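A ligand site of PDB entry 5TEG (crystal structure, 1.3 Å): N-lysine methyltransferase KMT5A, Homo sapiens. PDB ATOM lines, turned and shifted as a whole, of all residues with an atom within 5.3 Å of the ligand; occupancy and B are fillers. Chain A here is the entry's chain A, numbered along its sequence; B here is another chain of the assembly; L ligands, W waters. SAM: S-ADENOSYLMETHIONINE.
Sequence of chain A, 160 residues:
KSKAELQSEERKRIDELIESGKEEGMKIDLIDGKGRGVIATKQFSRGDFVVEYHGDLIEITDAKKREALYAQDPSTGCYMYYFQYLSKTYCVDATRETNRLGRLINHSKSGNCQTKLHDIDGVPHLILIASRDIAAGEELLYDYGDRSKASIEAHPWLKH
The side-chain hydroxyl (OH) of Tyr 79 lies within hydrogen-bond range of an oxygen (O) of the ligand. The backbone carbonyl oxygen of Lys 34 lies within hydrogen-bond range of a nitrogen (N) of the ligand (2.7 Å). A ring nitrogen (NE2) of His 3 of chain B sits at hydrogen-bond distance from an oxygen (O3') of the ligand. N of Arg 36 is in hydrogen-bond range of OXT of the ligand (2.9 Å). O of Arg 36 sits at hydrogen-bond distance from N of the ligand, 2.8 Å away. NH2 of Arg 36 is in salt-bridge range of O of the ligand (2.9 Å). OD1 of Asn 106 is in hydrogen-bond range of N of the ligand, 2.9 Å away. N of His 107 lies within hydrogen-bond range of N7 of the ligand, at 2.9 Å. The backbone carbonyl oxygen of His 107 lies within hydrogen-bond range of a nitrogen (N6) of the ligand.
The side-chain hydroxyl of Tyr 79 is in hydrogen-bond range of the guanidinium group of Arg 36 (3.4 Å). The side-chain hydroxyl (OH) of Tyr 53 is in hydrogen-bond range of the backbone carbonyl oxygen (O) of Tyr 79, at 2.7 Å. SG of Cys 78 is in hydrogen-bond range of N of His 3 of chain B (3.5 Å). The backbone carbonyl oxygen (O) of Arg 36 is in hydrogen-bond range of the side-chain amide nitrogen (ND2) of Asn 106, 3.0 Å away. The guanidinium group (NH1) of Arg 36 is in salt-bridge range of the side-chain carboxylate (OE1) of Glu 97, at 3.0 Å. A ring nitrogen (ND1) of His 107 is in hydrogen-bond range of the backbone NH (N) of Tyr 144, 2.9 Å away. NH1 of Arg 103 lies within salt-bridge range of OE1 of Glu 97 (3.0 Å). OH of Tyr 144 lies within hydrogen-bond range of O of Ile 105, at 2.8 Å.
The backbone carbonyl oxygen (O) of Arg 103 sits close to a sulfur (SD) of the ligand (3.7 Å). OH of Tyr 144 sits close to SD of the ligand (3.8 Å). Gly 33 touches the ligand. Gly 35 touches the ligand. Cys 78 touches the ligand. Leu 104 touches the ligand (O to CB, 3.4 Å). Ile 105 touches the ligand (O to CG, 3.6 Å). Trp 157 touches the ligand (CB to N1, 3.3 Å). NLE 5 of chain B touches the ligand. Within 4 Å of the ligand: Gly 33, Lys 34, Gly 35, Arg 36, Cys 78, Tyr 79, Arg 103, Leu 104, Ile 105, Asn 106, His 107, Tyr 144, Trp 157, His 3 of chain B and NLE 5 of chain B. The nearest printed residue that does not touch the ligand is Tyr 53 (4.6 Å).
Water W5 lies within hydrogen-bond range of O3' of the ligand (2.6 Å) and N of Cys 78 (2.9 Å). Water W2 bridges N of the ligand (3.1 Å) and O of Lys 34 (3.4 Å). Water W1 lies within hydrogen-bond range of the backbone carbonyl oxygen (O) of Trp 157 and a nitrogen (N6) of the ligand. Water W4 lies within hydrogen-bond range of O of His 107 (2.7 Å), NZ of Lys 34 (3.0 Å) and N6 of the ligand (3.4 Å).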
ATOM      1  N   GLY A  33      15.706  21.234  12.729  1.00  0.00           N
ATOM      2  CA  GLY A  33      15.367  22.588  13.135  1.00  0.00           C
ATOM      3  C   GLY A  33      15.132  22.816  14.612  1.00  0.00           C
ATOM      4  O   GLY A  33      14.740  23.912  14.991  1.00  0.00           O
ATOM      5  N   LYS A  34      15.335  21.793  15.451  1.00  0.00           N
ATOM      6  CA  LYS A  34      14.997  21.949  16.876  1.00  0.00           C
ATOM      7  C   LYS A  34      16.154  21.679  17.809  1.00  0.00           C
ATOM      8  O   LYS A  34      15.994  21.877  19.020  1.00  0.00           O
ATOM      9  CB  LYS A  34      13.805  21.034  17.271  1.00  0.00           C
ATOM     10  CG  LYS A  34      12.572  21.220  16.395  1.00  0.00           C
ATOM     11  CD  LYS A  34      11.341  20.546  17.006  1.00  0.00           C
ATOM     12  CE  LYS A  34      10.266  20.459  15.942  1.00  0.00           C
ATOM     13  NZ  LYS A  34       9.342  19.325  16.173  1.00  0.00           N
ATOM     14  N   GLY A  35      17.312  21.255  17.302  1.00  0.00           N
ATOM     15  CA  GLY A  35      18.410  20.832  18.159  1.00  0.00           C
ATOM     16  C   GLY A  35      18.201  19.383  18.581  1.00  0.00           C
ATOM     17  O   GLY A  35      17.854  18.547  17.748  1.00  0.00           O
ATOM     18  N   ARG A  36      18.398  19.069  19.854  1.00  0.00           N
ATOM     19  CA  ARG A  36      18.121  17.736  20.356  1.00  0.00           C
ATOM     20  C   ARG A  36      16.642  17.666  20.675  1.00  0.00           C
ATOM     21  O   ARG A  36      15.999  18.660  21.015  1.00  0.00           O
ATOM     22  CB  ARG A  36      18.877  17.481  21.673  1.00  0.00           C
ATOM     23  CG  ARG A  36      20.396  17.603  21.586  1.00  0.00           C
ATOM     24  CD  ARG A  36      21.028  17.637  22.975  1.00  0.00           C
ATOM     25  NE  ARG A  36      20.750  18.904  23.676  1.00  0.00           N
ATOM     26  CZ  ARG A  36      21.212  19.189  24.888  1.00  0.00           C
ATOM     27  NH1 ARG A  36      21.963  18.317  25.543  1.00  0.00           N
ATOM     28  NH2 ARG A  36      20.932  20.356  25.450  1.00  0.00           N
ATOM     29  N   GLY A  37      16.103  16.470  20.592  1.00  0.00           N
ATOM     30  CA  GLY A  37      14.755  16.149  21.034  1.00  0.00           C
ATOM     31  C   GLY A  37      14.740  14.724  21.543  1.00  0.00           C
ATOM     32  O   GLY A  37      15.780  14.072  21.676  1.00  0.00           O
ATOM     33  N   TYR A  53       9.611  16.265  34.251  1.00  0.00           N
ATOM     34  CA  TYR A  53      10.384  17.443  33.849  1.00  0.00           C
ATOM     35  C   TYR A  53      11.225  17.727  35.092  1.00  0.00           C
ATOM     36  O   TYR A  53      10.781  18.347  36.068  1.00  0.00           O
ATOM     37  CB  TYR A  53       9.519  18.656  33.442  1.00  0.00           C
ATOM     38  CG  TYR A  53      10.398  19.767  32.901  1.00  0.00           C
ATOM     39  CD1 TYR A  53      10.985  20.684  33.751  1.00  0.00           C
ATOM     40  CD2 TYR A  53      10.686  19.852  31.548  1.00  0.00           C
ATOM     41  CE1 TYR A  53      11.791  21.705  33.275  1.00  0.00           C
ATOM     42  CE2 TYR A  53      11.532  20.846  31.057  1.00  0.00           C
ATOM     43  CZ  TYR A  53      12.070  21.767  31.921  1.00  0.00           C
ATOM     44  OH  TYR A  53      12.904  22.724  31.396  1.00  0.00           O
ATOM     45  N   CYS A  78      16.839  28.032  27.294  1.00  0.00           N
ATOM     46  CA  CYS A  78      15.670  28.307  28.119  1.00  0.00           C
ATOM     47  C   CYS A  78      15.035  27.022  28.628  1.00  0.00           C
ATOM     48  O   CYS A  78      14.422  26.280  27.839  1.00  0.00           O
ATOM     49  CB  CYS A  78      14.652  29.148  27.352  1.00  0.00           C
ATOM     50  SG  CYS A  78      15.329  30.707  26.735  1.00  0.00           S
ATOM     51  N   TYR A  79      15.190  26.799  29.945  1.00  0.00           N
ATOM     52  CA  TYR A  79      14.751  25.553  30.574  1.00  0.00           C
ATOM     53  C   TYR A  79      13.990  25.800  31.868  1.00  0.00           C
ATOM     54  O   TYR A  79      13.907  24.879  32.687  1.00  0.00           O
ATOM     55  CB  TYR A  79      15.979  24.682  30.889  1.00  0.00           C
ATOM     56  CG  TYR A  79      16.751  24.221  29.683  1.00  0.00           C
ATOM     57  CD1 TYR A  79      16.431  23.026  29.031  1.00  0.00           C
ATOM     58  CD2 TYR A  79      17.831  24.974  29.191  1.00  0.00           C
ATOM     59  CE1 TYR A  79      17.191  22.566  27.950  1.00  0.00           C
ATOM     60  CE2 TYR A  79      18.553  24.539  28.074  1.00  0.00           C
ATOM     61  CZ  TYR A  79      18.218  23.351  27.466  1.00  0.00           C
ATOM     62  OH  TYR A  79      18.954  22.939  26.386  1.00  0.00           O
ATOM     63  N   GLU A  97      23.053  20.963  32.505  1.00  0.00           N
ATOM     64  CA  GLU A  97      23.065  19.793  31.644  1.00  0.00           C
ATOM     65  C   GLU A  97      23.223  18.536  32.459  1.00  0.00           C
ATOM     66  O   GLU A  97      24.209  18.357  33.184  1.00  0.00           O
ATOM     67  CB  GLU A  97      24.184  19.940  30.598  1.00  0.00           C
ATOM     68  CG  GLU A  97      23.824  20.955  29.519  1.00  0.00           C
ATOM     69  CD  GLU A  97      22.696  20.549  28.595  1.00  0.00           C
ATOM     70  OE1 GLU A  97      22.552  19.343  28.302  1.00  0.00           O
ATOM     71  OE2 GLU A  97      22.029  21.467  28.050  1.00  0.00           O
ATOM     72  N   ARG A 103      13.813  17.524  30.093  1.00  0.00           N
ATOM     73  CA  ARG A 103      14.313  18.825  29.707  1.00  0.00           C
ATOM     74  C   ARG A 103      14.724  18.915  28.234  1.00  0.00           C
ATOM     75  O   ARG A 103      14.991  20.022  27.731  1.00  0.00           O
ATOM     76  CB  ARG A 103      15.488  19.238  30.602  1.00  0.00           C
ATOM     77  CG  ARG A 103      16.682  18.268  30.432  1.00  0.00           C
ATOM     78  CD  ARG A 103      17.826  18.545  31.389  1.00  0.00           C
ATOM     79  NE  ARG A 103      18.434  19.842  31.172  1.00  0.00           N
ATOM     80  CZ  ARG A 103      19.360  20.109  30.257  1.00  0.00           C
ATOM     81  NH1 ARG A 103      19.834  19.140  29.482  1.00  0.00           N
ATOM     82  NH2 ARG A 103      19.820  21.351  30.108  1.00  0.00           N
ATOM     83  N   LEU A 104      14.731  17.784  27.497  1.00  0.00           N
ATOM     84  CA  LEU A 104      15.078  17.785  26.088  1.00  0.00           C
ATOM     85  C   LEU A 104      13.911  17.715  25.164  1.00  0.00           C
ATOM     86  O   LEU A 104      14.074  17.720  23.953  1.00  0.00           O
ATOM     87  CB  LEU A 104      16.069  16.668  25.765  1.00  0.00           C
ATOM     88  CG  LEU A 104      17.405  16.758  26.474  1.00  0.00           C
ATOM     89  CD1 LEU A 104      18.309  15.622  26.035  1.00  0.00           C
ATOM     90  CD2 LEU A 104      18.065  18.137  26.313  1.00  0.00           C
ATOM     91  N   ILE A 105      12.703  17.712  25.702  1.00  0.00           N
ATOM     92  CA  ILE A 105      11.489  17.598  24.917  1.00  0.00           C
ATOM     93  C   ILE A 105      11.110  18.950  24.308  1.00  0.00           C
ATOM     94  O   ILE A 105      11.118  19.969  25.016  1.00  0.00           O
ATOM     95  CB  ILE A 105      10.365  16.953  25.719  1.00  0.00           C
ATOM     96  CG1 ILE A 105      10.747  15.479  26.004  1.00  0.00           C
ATOM     97  CG2 ILE A 105       9.034  17.005  24.921  1.00  0.00           C
ATOM     98  CD1 ILE A 105       9.819  14.778  26.997  1.00  0.00           C
ATOM     99  N   ASN A 106      10.814  18.975  23.022  1.00  0.00           N
ATOM    100  CA  ASN A 106      10.508  20.186  22.280  1.00  0.00           C
ATOM    101  C   ASN A 106       9.030  20.608  22.341  1.00  0.00           C
ATOM    102  O   ASN A 106       8.191  19.881  22.897  1.00  0.00           O
ATOM    103  CB  ASN A 106      11.018  20.045  20.865  1.00  0.00           C
ATOM    104  CG  ASN A 106      12.529  20.068  20.800  1.00  0.00           C
ATOM    105  OD1 ASN A 106      13.193  20.911  21.452  1.00  0.00           O
ATOM    106  ND2 ASN A 106      13.117  19.058  20.157  1.00  0.00           N
ATOM    107  N   HIS A 107       8.735  21.769  21.783  1.00  0.00           N
ATOM    108  CA  HIS A 107       7.421  22.373  21.821  1.00  0.00           C
ATOM    109  C   HIS A 107       6.562  22.132  20.622  1.00  0.00           C
ATOM    110  O   HIS A 107       7.048  22.167  19.486  1.00  0.00           O
ATOM    111  CB  HIS A 107       7.601  23.902  21.931  1.00  0.00           C
ATOM    112  CG  HIS A 107       6.362  24.710  21.638  1.00  0.00           C
ATOM    113  ND1 HIS A 107       5.419  24.998  22.619  1.00  0.00           N
ATOM    114  CD2 HIS A 107       5.955  25.281  20.470  1.00  0.00           C
ATOM    115  CE1 HIS A 107       4.459  25.653  22.009  1.00  0.00           C
ATOM    116  NE2 HIS A 107       4.755  25.875  20.720  1.00  0.00           N
ATOM    117  N   SER A 108       5.274  21.960  20.871  1.00  0.00           N
ATOM    118  CA  SER A 108       4.253  22.025  19.848  1.00  0.00           C
ATOM    119  C   SER A 108       2.955  22.373  20.528  1.00  0.00           C
ATOM    120  O   SER A 108       2.704  21.893  21.625  1.00  0.00           O
ATOM    121  CB  SER A 108       4.074  20.700  19.118  1.00  0.00           C
ATOM    122  OG  SER A 108       2.974  20.822  18.209  1.00  0.00           O
ATOM    123  N   TYR A 144       4.734  24.543  25.379  1.00  0.00           N
ATOM    124  CA  TYR A 144       5.478  25.245  26.408  1.00  0.00           C
ATOM    125  C   TYR A 144       4.625  26.318  27.086  1.00  0.00           C
ATOM    126  O   TYR A 144       4.932  26.704  28.203  1.00  0.00           O
ATOM    127  CB  TYR A 144       6.672  25.946  25.773  1.00  0.00           C
ATOM    128  CG  TYR A 144       7.852  25.054  25.414  1.00  0.00           C
ATOM    129  CD1 TYR A 144       7.788  23.667  25.557  1.00  0.00           C
ATOM    130  CD2 TYR A 144       9.019  25.605  24.918  1.00  0.00           C
ATOM    131  CE1 TYR A 144       8.880  22.851  25.266  1.00  0.00           C
ATOM    132  CE2 TYR A 144      10.115  24.805  24.601  1.00  0.00           C
ATOM    133  CZ  TYR A 144      10.046  23.441  24.783  1.00  0.00           C
ATOM    134  OH  TYR A 144      11.148  22.683  24.457  1.00  0.00           O
ATOM    135  N   HIS A 155      11.371  33.778  19.132  1.00  0.00           N
ATOM    136  CA  HIS A 155      11.313  32.315  18.992  1.00  0.00           C
ATOM    137  C   HIS A 155      10.025  31.998  18.208  1.00  0.00           C
ATOM    138  O   HIS A 155       9.001  31.581  18.789  1.00  0.00           O
ATOM    139  CB  HIS A 155      11.274  31.675  20.401  1.00  0.00           C
ATOM    140  CG  HIS A 155      12.387  32.072  21.286  1.00  0.00           C
ATOM    141  ND1 HIS A 155      13.632  31.471  21.191  1.00  0.00           N
ATOM    142  CD2 HIS A 155      12.453  33.053  22.213  1.00  0.00           C
ATOM    143  CE1 HIS A 155      14.410  32.095  22.064  1.00  0.00           C
ATOM    144  NE2 HIS A 155      13.734  33.058  22.706  1.00  0.00           N
ATOM    145  N   TRP A 157       8.869  29.709  16.361  1.00  0.00           N
ATOM    146  CA  TRP A 157       8.305  28.369  16.443  1.00  0.00           C
ATOM    147  C   TRP A 157       7.302  28.234  17.595  1.00  0.00           C
ATOM    148  O   TRP A 157       6.545  27.274  17.615  1.00  0.00           O
ATOM    149  CB  TRP A 157       9.440  27.363  16.602  1.00  0.00           C
ATOM    150  CG  TRP A 157      10.435  27.755  17.642  1.00  0.00           C
ATOM    151  CD1 TRP A 157      11.608  28.409  17.443  1.00  0.00           C
ATOM    152  CD2 TRP A 157      10.320  27.534  19.052  1.00  0.00           C
ATOM    153  NE1 TRP A 157      12.267  28.589  18.630  1.00  0.00           N
ATOM    154  CE2 TRP A 157      11.488  28.067  19.638  1.00  0.00           C
ATOM    155  CE3 TRP A 157       9.384  26.855  19.867  1.00  0.00           C
ATOM    156  CZ2 TRP A 157      11.710  28.017  21.019  1.00  0.00           C
ATOM    157  CZ3 TRP A 157       9.600  26.829  21.228  1.00  0.00           C
ATOM    158  CH2 TRP A 157      10.754  27.394  21.802  1.00  0.00           C
ATOM    159  N   HIS B   3      12.639  32.873  26.337  1.00  0.00           N
ATOM    160  CA  HIS B   3      11.233  32.485  26.554  1.00  0.00           C
ATOM    161  C   HIS B   3      11.181  31.691  27.852  1.00  0.00           C
ATOM    162  O   HIS B   3      12.220  31.286  28.391  1.00  0.00           O
ATOM    163  CB  HIS B   3      10.652  31.658  25.385  1.00  0.00           C
ATOM    164  CG  HIS B   3      11.229  30.280  25.266  1.00  0.00           C
ATOM    165  ND1 HIS B   3      10.741  29.210  26.010  1.00  0.00           N
ATOM    166  CD2 HIS B   3      12.226  29.818  24.475  1.00  0.00           C
ATOM    167  CE1 HIS B   3      11.494  28.161  25.696  1.00  0.00           C
ATOM    168  NE2 HIS B   3      12.404  28.491  24.777  1.00  0.00           N
ATOM    169  N   NLE B   5       8.635  28.526  30.055  1.00  0.00           N
ATOM    170  CA  NLE B   5       7.664  27.463  29.942  1.00  0.00           C
ATOM    171  C   NLE B   5       6.724  27.713  31.127  1.00  0.00           C
ATOM    172  O   NLE B   5       7.193  28.071  32.229  1.00  0.00           O
ATOM    173  CB  NLE B   5       8.225  26.061  30.042  1.00  0.00           C
ATOM    174  CG  NLE B   5       9.187  25.769  28.848  1.00  0.00           C
ATOM    175  CD  NLE B   5       9.984  24.528  29.262  1.00  0.00           C
ATOM    176  CE  NLE B   5      11.147  24.194  28.363  1.00  0.00           C
HETATM  177  N   SAM L   1      16.013  21.349  21.695  1.00  0.00           N
HETATM  178  CA  SAM L   1      16.516  21.562  23.070  1.00  0.00           C
HETATM  179  C   SAM L   1      18.043  21.205  23.237  1.00  0.00           C
HETATM  180  O   SAM L   1      18.521  21.430  24.322  1.00  0.00           O
HETATM  181  OXT SAM L   1      18.624  20.718  22.236  1.00  0.00           O
HETATM  182  CB  SAM L   1      15.694  20.725  24.085  1.00  0.00           C
HETATM  183  CG  SAM L   1      14.390  21.470  24.543  1.00  0.00           C
HETATM  184  SD  SAM L   1      14.774  23.005  25.478  1.00  0.00           S
HETATM  185  CE  SAM L   1      13.682  22.843  26.837  1.00  0.00           C
HETATM  186  C5' SAM L   1      14.013  24.400  24.648  1.00  0.00           C
HETATM  187  C4' SAM L   1      14.695  24.897  23.388  1.00  0.00           C
HETATM  188  O4' SAM L   1      14.486  23.904  22.373  1.00  0.00           O
HETATM  189  C3' SAM L   1      14.009  26.131  22.765  1.00  0.00           C
HETATM  190  O3' SAM L   1      14.456  27.326  23.378  1.00  0.00           O
HETATM  191  C2' SAM L   1      14.488  26.010  21.284  1.00  0.00           C
HETATM  192  O2' SAM L   1      15.872  26.306  21.207  1.00  0.00           O
HETATM  193  C1' SAM L   1      14.338  24.469  21.099  1.00  0.00           C
HETATM  194  N9  SAM L   1      12.982  24.199  20.628  1.00  0.00           N
HETATM  195  C8  SAM L   1      11.899  23.610  21.326  1.00  0.00           C
HETATM  196  N7  SAM L   1      10.849  23.421  20.578  1.00  0.00           N
HETATM  197  C5  SAM L   1      11.179  23.886  19.321  1.00  0.00           C
HETATM  198  C6  SAM L   1      10.462  23.943  18.157  1.00  0.00           C
HETATM  199  N6  SAM L   1       9.176  23.542  18.011  1.00  0.00           N
HETATM  200  N1  SAM L   1      11.100  24.509  17.049  1.00  0.00           N
HETATM  201  C2  SAM L   1      12.359  24.986  17.190  1.00  0.00           C
HETATM  202  N3  SAM L   1      13.133  24.964  18.281  1.00  0.00           N
HETATM  203  C4  SAM L   1      12.500  24.399  19.352  1.00  0.00           C
HETATM  204  O   HOH W   1       6.842  24.874  16.198  1.00  0.00           O
HETATM  205  O   HOH W   2      17.728  23.814  21.135  1.00  0.00           O
HETATM  206  O   HOH W   3      10.786  24.578  14.313  1.00  0.00           O
HETATM  207  O   HOH W   4       7.058  21.083  16.968  1.00  0.00           O
HETATM  208  O   HOH W   5      16.830  27.502  24.427  1.00  0.00           O
HETATM  209  O   HOH W   6      15.979  26.182  17.648  1.00  0.00           O
